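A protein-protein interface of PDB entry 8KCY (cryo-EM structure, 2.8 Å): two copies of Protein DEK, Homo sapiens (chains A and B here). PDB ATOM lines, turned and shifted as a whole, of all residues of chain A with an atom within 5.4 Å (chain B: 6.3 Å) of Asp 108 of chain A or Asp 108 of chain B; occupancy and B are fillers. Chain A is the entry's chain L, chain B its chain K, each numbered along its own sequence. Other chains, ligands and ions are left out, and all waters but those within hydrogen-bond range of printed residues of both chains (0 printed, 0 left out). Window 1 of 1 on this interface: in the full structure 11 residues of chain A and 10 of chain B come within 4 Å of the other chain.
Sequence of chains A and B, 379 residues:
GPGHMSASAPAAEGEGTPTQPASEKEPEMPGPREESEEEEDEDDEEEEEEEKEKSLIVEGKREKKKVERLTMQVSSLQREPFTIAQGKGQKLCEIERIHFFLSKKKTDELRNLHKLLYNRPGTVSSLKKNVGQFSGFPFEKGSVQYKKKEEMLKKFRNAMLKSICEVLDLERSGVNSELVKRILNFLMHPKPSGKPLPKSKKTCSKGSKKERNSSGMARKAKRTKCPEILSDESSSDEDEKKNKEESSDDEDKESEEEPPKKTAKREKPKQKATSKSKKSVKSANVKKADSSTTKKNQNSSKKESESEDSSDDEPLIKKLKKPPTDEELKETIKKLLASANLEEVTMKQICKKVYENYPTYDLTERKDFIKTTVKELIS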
ATOM      1  N   LYS A 106      -9.748   6.681  -9.666  1.00  0.00           N
ATOM      2  CA  LYS A 106      -8.905   6.205 -10.805  1.00  0.00           C
ATOM      3  C   LYS A 106      -8.890   4.671 -10.888  1.00  0.00           C
ATOM      4  O   LYS A 106      -9.397   4.026  -9.949  1.00  0.00           O
ATOM      5  CB  LYS A 106      -7.474   6.743 -10.685  1.00  0.00           C
ATOM      6  CG  LYS A 106      -7.233   8.111 -11.310  1.00  0.00           C
ATOM      7  CD  LYS A 106      -7.568   9.271 -10.395  1.00  0.00           C
ATOM      8  CE  LYS A 106      -7.486  10.616 -11.085  1.00  0.00           C
ATOM      9  NZ  LYS A 106      -7.875  11.719 -10.177  1.00  0.00           N
ATOM     10  N   THR A 107      -8.317   4.117 -11.968  1.00  0.00           N
ATOM     11  CA  THR A 107      -8.292   2.639 -12.147  1.00  0.00           C
ATOM     12  C   THR A 107      -7.587   2.042 -10.928  1.00  0.00           C
ATOM     13  O   THR A 107      -8.131   1.103 -10.333  1.00  0.00           O
ATOM     14  CB  THR A 107      -7.633   2.275 -13.484  1.00  0.00           C
ATOM     15  OG1 THR A 107      -8.413   2.858 -14.529  1.00  0.00           O
ATOM     16  CG2 THR A 107      -7.511   0.785 -13.717  1.00  0.00           C
ATOM     17  N   ASP A 108      -6.439   2.606 -10.550  1.00  0.00           N
ATOM     18  CA  ASP A 108      -5.623   2.082  -9.419  1.00  0.00           C
ATOM     19  C   ASP A 108      -6.483   1.642  -8.229  1.00  0.00           C
ATOM     20  O   ASP A 108      -6.370   0.460  -7.846  1.00  0.00           O
ATOM     21  CB  ASP A 108      -4.604   3.136  -8.980  1.00  0.00           C
ATOM     22  CG  ASP A 108      -3.760   3.676 -10.122  1.00  0.00           C
ATOM     23  OD1 ASP A 108      -3.208   4.783  -9.965  1.00  0.00           O
ATOM     24  OD2 ASP A 108      -3.659   2.987 -11.156  1.00  0.00           O
ATOM     25  N   GLU A 109      -7.298   2.538  -7.661  1.00  0.00           N
ATOM     26  CA  GLU A 109      -8.046   2.218  -6.449  1.00  0.00           C
ATOM     27  C   GLU A 109      -8.894   0.961  -6.617  1.00  0.00           C
ATOM     28  O   GLU A 109      -9.024   0.157  -5.695  1.00  0.00           O
ATOM     29  CB  GLU A 109      -8.934   3.397  -6.042  1.00  0.00           C
ATOM     30  CG  GLU A 109      -9.858   3.102  -4.872  1.00  0.00           C
ATOM     31  CD  GLU A 109      -9.108   2.633  -3.641  1.00  0.00           C
ATOM     32  OE1 GLU A 109      -9.765   2.324  -2.625  1.00  0.00           O
ATOM     33  OE2 GLU A 109      -7.861   2.575  -3.689  1.00  0.00           O
ATOM     34  N   LEU A 110      -9.537   0.835  -7.785  1.00  0.00           N
ATOM     35  CA  LEU A 110     -10.489  -0.291  -8.003  1.00  0.00           C
ATOM     36  C   LEU A 110      -9.758  -1.631  -8.154  1.00  0.00           C
ATOM     37  O   LEU A 110     -10.456  -2.654  -8.224  1.00  0.00           O
ATOM     38  CB  LEU A 110     -11.336   0.002  -9.247  1.00  0.00           C
ATOM     39  CG  LEU A 110     -12.578   0.867  -9.027  1.00  0.00           C
ATOM     40  CD1 LEU A 110     -13.517   0.237  -8.011  1.00  0.00           C
ATOM     41  CD2 LEU A 110     -12.206   2.282  -8.611  1.00  0.00           C
ATOM     42  N   ARG A 111      -8.422  -1.633  -8.202  1.00  0.00           N
ATOM     43  CA  ARG A 111      -7.692  -2.930  -8.252  1.00  0.00           C
ATOM     44  C   ARG A 111      -7.971  -3.707  -6.961  1.00  0.00           C
ATOM     45  O   ARG A 111      -8.315  -4.898  -7.062  1.00  0.00           O
ATOM     46  CB  ARG A 111      -6.192  -2.714  -8.473  1.00  0.00           C
ATOM     47  CG  ARG A 111      -5.848  -2.174  -9.853  1.00  0.00           C
ATOM     48  CD  ARG A 111      -4.414  -2.460 -10.256  1.00  0.00           C
ATOM     49  NE  ARG A 111      -4.122  -3.887 -10.270  1.00  0.00           N
ATOM     50  CZ  ARG A 111      -4.300  -4.691 -11.313  1.00  0.00           C
ATOM     51  NH1 ARG A 111      -4.775  -4.214 -12.451  1.00  0.00           N
ATOM     52  NH2 ARG A 111      -4.001  -5.974 -11.215  1.00  0.00           N
ATOM     53  N   ASN A 112      -7.854  -3.046  -5.804  1.00  0.00           N
ATOM     54  CA  ASN A 112      -8.109  -3.708  -4.496  1.00  0.00           C
ATOM     55  C   ASN A 112      -9.593  -4.072  -4.371  1.00  0.00           C
ATOM     56  O   ASN A 112      -9.884  -5.153  -3.821  1.00  0.00           O
ATOM     57  CB  ASN A 112      -7.653  -2.840  -3.320  1.00  0.00           C
ATOM     58  CG  ASN A 112      -6.147  -2.779  -3.173  1.00  0.00           C
ATOM     59  OD1 ASN A 112      -5.420  -3.499  -3.855  1.00  0.00           O
ATOM     60  ND2 ASN A 112      -5.669  -1.926  -2.283  1.00  0.00           N
ATOM     61  N   LYS B 105       0.032   8.283   0.107  1.00  0.00           N
ATOM     62  CA  LYS B 105      -0.492   7.395  -0.929  1.00  0.00           C
ATOM     63  C   LYS B 105      -0.618   5.955  -0.433  1.00  0.00           C
ATOM     64  O   LYS B 105      -0.154   5.621   0.656  1.00  0.00           O
ATOM     65  CB  LYS B 105       0.394   7.445  -2.176  1.00  0.00           C
ATOM     66  CG  LYS B 105       0.281   8.738  -2.967  1.00  0.00           C
ATOM     67  CD  LYS B 105      -1.119   8.913  -3.535  1.00  0.00           C
ATOM     68  CE  LYS B 105      -1.219  10.172  -4.379  1.00  0.00           C
ATOM     69  NZ  LYS B 105      -2.582  10.347  -4.953  1.00  0.00           N
ATOM     70  N   LYS B 106      -1.240   5.110  -1.270  1.00  0.00           N
ATOM     71  CA  LYS B 106      -1.419   3.668  -0.938  1.00  0.00           C
ATOM     72  C   LYS B 106      -0.816   2.809  -2.058  1.00  0.00           C
ATOM     73  O   LYS B 106      -0.477   3.384  -3.111  1.00  0.00           O
ATOM     74  CB  LYS B 106      -2.901   3.327  -0.751  1.00  0.00           C
ATOM     75  CG  LYS B 106      -3.557   3.872   0.513  1.00  0.00           C
ATOM     76  CD  LYS B 106      -4.089   5.281   0.366  1.00  0.00           C
ATOM     77  CE  LYS B 106      -4.606   5.862   1.664  1.00  0.00           C
ATOM     78  NZ  LYS B 106      -5.073   7.257   1.492  1.00  0.00           N
ATOM     79  N   THR B 107      -0.721   1.488  -1.877  1.00  0.00           N
ATOM     80  CA  THR B 107      -0.015   0.608  -2.860  1.00  0.00           C
ATOM     81  C   THR B 107      -0.669   0.575  -4.254  1.00  0.00           C
ATOM     82  O   THR B 107      -0.177  -0.204  -5.092  1.00  0.00           O
ATOM     83  CB  THR B 107       0.123  -0.813  -2.290  1.00  0.00           C
ATOM     84  OG1 THR B 107       1.091  -1.534  -3.053  1.00  0.00           O
ATOM     85  CG2 THR B 107      -1.186  -1.572  -2.276  1.00  0.00           C
ATOM     86  N   ASP B 108      -1.703   1.381  -4.519  1.00  0.00           N
ATOM     87  CA  ASP B 108      -2.420   1.304  -5.825  1.00  0.00           C
ATOM     88  C   ASP B 108      -1.809   2.284  -6.836  1.00  0.00           C
ATOM     89  O   ASP B 108      -1.586   1.870  -7.988  1.00  0.00           O
ATOM     90  CB  ASP B 108      -3.915   1.565  -5.638  1.00  0.00           C
ATOM     91  CG  ASP B 108      -4.603   0.549  -4.743  1.00  0.00           C
ATOM     92  OD1 ASP B 108      -4.973   0.921  -3.613  1.00  0.00           O
ATOM     93  OD2 ASP B 108      -4.773  -0.603  -5.189  1.00  0.00           O
ATOM     94  N   GLU B 109      -1.664   3.552  -6.434  1.00  0.00           N
ATOM     95  CA  GLU B 109      -1.099   4.594  -7.332  1.00  0.00           C
ATOM     96  C   GLU B 109       0.368   4.252  -7.582  1.00  0.00           C
ATOM     97  O   GLU B 109       0.833   4.445  -8.722  1.00  0.00           O
ATOM     98  CB  GLU B 109      -1.240   5.979  -6.698  1.00  0.00           C
ATOM     99  CG  GLU B 109      -2.674   6.358  -6.370  1.00  0.00           C
ATOM    100  CD  GLU B 109      -3.204   5.857  -5.037  1.00  0.00           C
ATOM    101  OE1 GLU B 109      -4.437   5.752  -4.896  1.00  0.00           O
ATOM    102  OE2 GLU B 109      -2.383   5.577  -4.140  1.00  0.00           O
ATOM    103  N   LEU B 110       1.059   3.765  -6.549  1.00  0.00           N
ATOM    104  CA  LEU B 110       2.466   3.323  -6.718  1.00  0.00           C
ATOM    105  C   LEU B 110       2.484   2.124  -7.671  1.00  0.00           C
ATOM    106  O   LEU B 110       3.468   1.987  -8.421  1.00  0.00           O
ATOM    107  CB  LEU B 110       3.035   2.944  -5.349  1.00  0.00           C
ATOM    108  CG  LEU B 110       3.577   4.084  -4.493  1.00  0.00           C
ATOM    109  CD1 LEU B 110       2.464   4.754  -3.704  1.00  0.00           C
ATOM    110  CD2 LEU B 110       4.661   3.578  -3.556  1.00  0.00           C
ATOM    111  N   ARG B 111       1.443   1.282  -7.631  1.00  0.00           N
ATOM    112  CA  ARG B 111       1.369   0.102  -8.539  1.00  0.00           C
ATOM    113  C   ARG B 111       1.338   0.602  -9.982  1.00  0.00           C
ATOM    114  O   ARG B 111       2.078   0.031 -10.810  1.00  0.00           O
ATOM    115  CB  ARG B 111       0.165  -0.789  -8.213  1.00  0.00           C
ATOM    116  CG  ARG B 111      -0.035  -1.962  -9.161  1.00  0.00           C
ATOM    117  CD  ARG B 111      -0.685  -3.139  -8.464  1.00  0.00           C
ATOM    118  NE  ARG B 111       0.263  -3.836  -7.606  1.00  0.00           N
ATOM    119  CZ  ARG B 111      -0.023  -4.904  -6.869  1.00  0.00           C
ATOM    120  NH1 ARG B 111      -1.245  -5.409  -6.871  1.00  0.00           N
ATOM    121  NH2 ARG B 111       0.918  -5.463  -6.131  1.00  0.00           N
ATOM    122  N   ASN B 112       0.546   1.643 -10.263  1.00  0.00           N
ATOM    123  CA  ASN B 112       0.578   2.212 -11.635  1.00  0.00           C
ATOM    124  C   ASN B 112       2.010   2.685 -11.904  1.00  0.00           C
ATOM    125  O   ASN B 112       2.555   2.291 -12.945  1.00  0.00           O
ATOM    126  CB  ASN B 112      -0.394   3.372 -11.827  1.00  0.00           C
ATOM    127  CG  ASN B 112      -0.593   3.763 -13.275  1.00  0.00           C
ATOM    128  OD1 ASN B 112      -0.278   3.001 -14.186  1.00  0.00           O
ATOM    129  ND2 ASN B 112      -1.132   4.951 -13.495  1.00  0.00           N
ATOM    130  N   LEU B 113       2.624   3.421 -10.965  1.00  0.00           N
ATOM    131  CA  LEU B 113       3.973   4.004 -11.237  1.00  0.00           C
ATOM    132  C   LEU B 113       5.013   2.911 -11.535  1.00  0.00           C
ATOM    133  O   LEU B 113       5.885   3.167 -12.385  1.00  0.00           O
ATOM    134  CB  LEU B 113       4.391   4.853 -10.031  1.00  0.00           C
ATOM    135  CG  LEU B 113       5.693   5.640 -10.190  1.00  0.00           C
ATOM    136  CD1 LEU B 113       5.635   6.548 -11.408  1.00  0.00           C
ATOM    137  CD2 LEU B 113       5.989   6.451  -8.939  1.00  0.00           C
ATOM    138  N   LEU B 127       6.374  -3.754  -4.205  1.00  0.00           N
ATOM    139  CA  LEU B 127       5.865  -2.537  -4.898  1.00  0.00           C
ATOM    140  C   LEU B 127       6.308  -1.300  -4.125  1.00  0.00           C
ATOM    141  O   LEU B 127       7.066  -0.489  -4.690  1.00  0.00           O
ATOM    142  CB  LEU B 127       4.336  -2.624  -4.909  1.00  0.00           C
ATOM    143  CG  LEU B 127       3.597  -1.800  -5.955  1.00  0.00           C
ATOM    144  CD1 LEU B 127       3.546  -0.336  -5.556  1.00  0.00           C
ATOM    145  CD2 LEU B 127       4.237  -1.974  -7.318  1.00  0.00           C
ATOM    146  N   LYS B 128       5.828  -1.168  -2.886  1.00  0.00           N
ATOM    147  CA  LYS B 128       6.238  -0.006  -2.035  1.00  0.00           C
ATOM    148  C   LYS B 128       7.767   0.188  -1.993  1.00  0.00           C
ATOM    149  O   LYS B 128       8.277   1.222  -2.563  1.00  0.00           O
ATOM    150  CB  LYS B 128       5.685  -0.184  -0.617  1.00  0.00           C
ATOM    151  CG  LYS B 128       5.741   1.053   0.268  1.00  0.00           C
ATOM    152  CD  LYS B 128       4.730   2.114  -0.113  1.00  0.00           C
ATOM    153  CE  LYS B 128       3.296   1.653   0.049  1.00  0.00           C
ATOM    154  NZ  LYS B 128       2.333   2.756  -0.185  1.00  0.00           N
ATOM    155  N   MET B 160      -4.679   8.322 -15.307  1.00  0.00           N
ATOM    156  CA  MET B 160      -3.506   7.640 -14.776  1.00  0.00           C
ATOM    157  C   MET B 160      -2.336   8.620 -14.786  1.00  0.00           C
ATOM    158  O   MET B 160      -1.692   8.834 -13.760  1.00  0.00           O
ATOM    159  CB  MET B 160      -3.173   6.405 -15.612  1.00  0.00           C
ATOM    160  CG  MET B 160      -4.274   5.359 -15.643  1.00  0.00           C
ATOM    161  SD  MET B 160      -3.832   3.912 -16.624  1.00  0.00           S
ATOM    162  CE  MET B 160      -5.292   2.897 -16.404  1.00  0.00           C
ATOM    163  N   SER B 163      -2.647  10.965 -12.065  1.00  0.00           N
ATOM    164  CA  SER B 163      -2.253  10.286 -10.820  1.00  0.00           C
ATOM    165  C   SER B 163      -0.733  10.120 -10.685  1.00  0.00           C
ATOM    166  O   SER B 163      -0.207  10.324  -9.594  1.00  0.00           O
ATOM    167  CB  SER B 163      -2.906   8.903 -10.709  1.00  0.00           C
ATOM    168  OG  SER B 163      -4.255   8.983 -10.282  1.00  0.00           O
ATOM    169  N   ILE B 164      -0.014   9.787 -11.764  1.00  0.00           N
ATOM    170  CA  ILE B 164       1.456   9.673 -11.763  1.00  0.00           C
ATOM    171  C   ILE B 164       2.102  11.045 -11.531  1.00  0.00           C
ATOM    172  O   ILE B 164       2.990  11.153 -10.689  1.00  0.00           O
ATOM    173  CB  ILE B 164       1.957   8.980 -13.056  1.00  0.00           C
ATOM    174  CG1 ILE B 164       1.561   7.482 -13.043  1.00  0.00           C
ATOM    175  CG2 ILE B 164       3.486   9.106 -13.212  1.00  0.00           C
ATOM    176  CD1 ILE B 164       1.659   6.800 -14.414  1.00  0.00           C
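Among the printed residues, pairs that only touch across the chains: Lys 106 of chain A with Ser 163 of chain B (3.3 Å), Asp 108 of chain A with Asn 112 of chain B (3.4 Å), Asp 108 of chain A with Glu 109 of chain B (3.4 Å), Thr 107 of chain A with Met 160 of chain B (3.6 Å) and Arg 111 of chain A with Arg 111 of chain B (3.95 Å).
The side-chain carboxylate (OE2) of Glu 109 of chain B sits at hydrogen-bond distance from the backbone NH (N) of Lys 106 of chain B (3.1 Å).
Asp 108 of chain A touches three residues of chain B. Printed residues of chain A within 4 Å of Asp 108 of chain B: Asp 108 (3.3 Å), Glu 109 (3.3 Å) and Asn 112 (3.2 Å). Of the printed residues of chain A, Glu 109 of chain B touches Asp 108 (3.4 Å). Printed residues of chain A within 4 Å of Arg 111 of chain B: Arg 111 (3.95 Å). Of the printed residues of chain B, Lys 106 of chain A touches Ser 163. Of the printed residues of chain A, Ser 163 of chain B touches Lys 106 (3.3 Å). Thr 107 of chain B touches none of the printed residues of chain A. The nearest residue of chain A that does not touch Asp 108 of chain B is Arg 111 of chain A (4.2 Å). The nearest printed residue of chain A that does not touch Glu 109 of chain B is Glu 109 of chain A (4.8 Å).
Asp 108 of chain B touches its own counterpart, Asp 108 of chain A. Asp 108 of chain A touches Glu 109 of chain B, and with the chains exchanged Glu 109 of chain A touches Asp 108 of chain B. Asp 108 of chain A touches Asn 112 of chain B, and with the chains exchanged Asn 112 of chain A touches Asp 108 of chain B. Arg 111 of chain B touches its own counterpart, Arg 111 of chain A. Of the 8 pairs that touch across the chains among the printed residues, 6 have their exchanged pair printed and touching as well.
The side-chain amide nitrogen of Asn 112 of chain A is in hydrogen-bond range of the side-chain carboxylate of Asp 108 of chain B, at 3.2 Å. The side-chain carboxylate (OE2) of Glu 109 of chain A lies close to the side-chain carboxylate (OD1) of Asp 108 of chain B (3.3 Å). O of Asp 108 of chain A sits close to OD2 of Asp 108 of chain B (3.3 Å).
Printed residues of chain A that touch a printed residue of chain B: Lys 106, Thr 107, Asp 108, Glu 109, Arg 111 and Asn 112. Printed residues of chain B that touch a printed residue of chain A: Asp 108, Glu 109, Arg 111, Asn 112, Met 160 and Ser 163. Hydrophobic or aromatic side chains of chain B that line the printed part of chain A: Met 160. Among the printed residues, no Asp or Glu carboxylate lies within 4 Å of a Lys or Arg side-chain nitrogen of the other chain.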
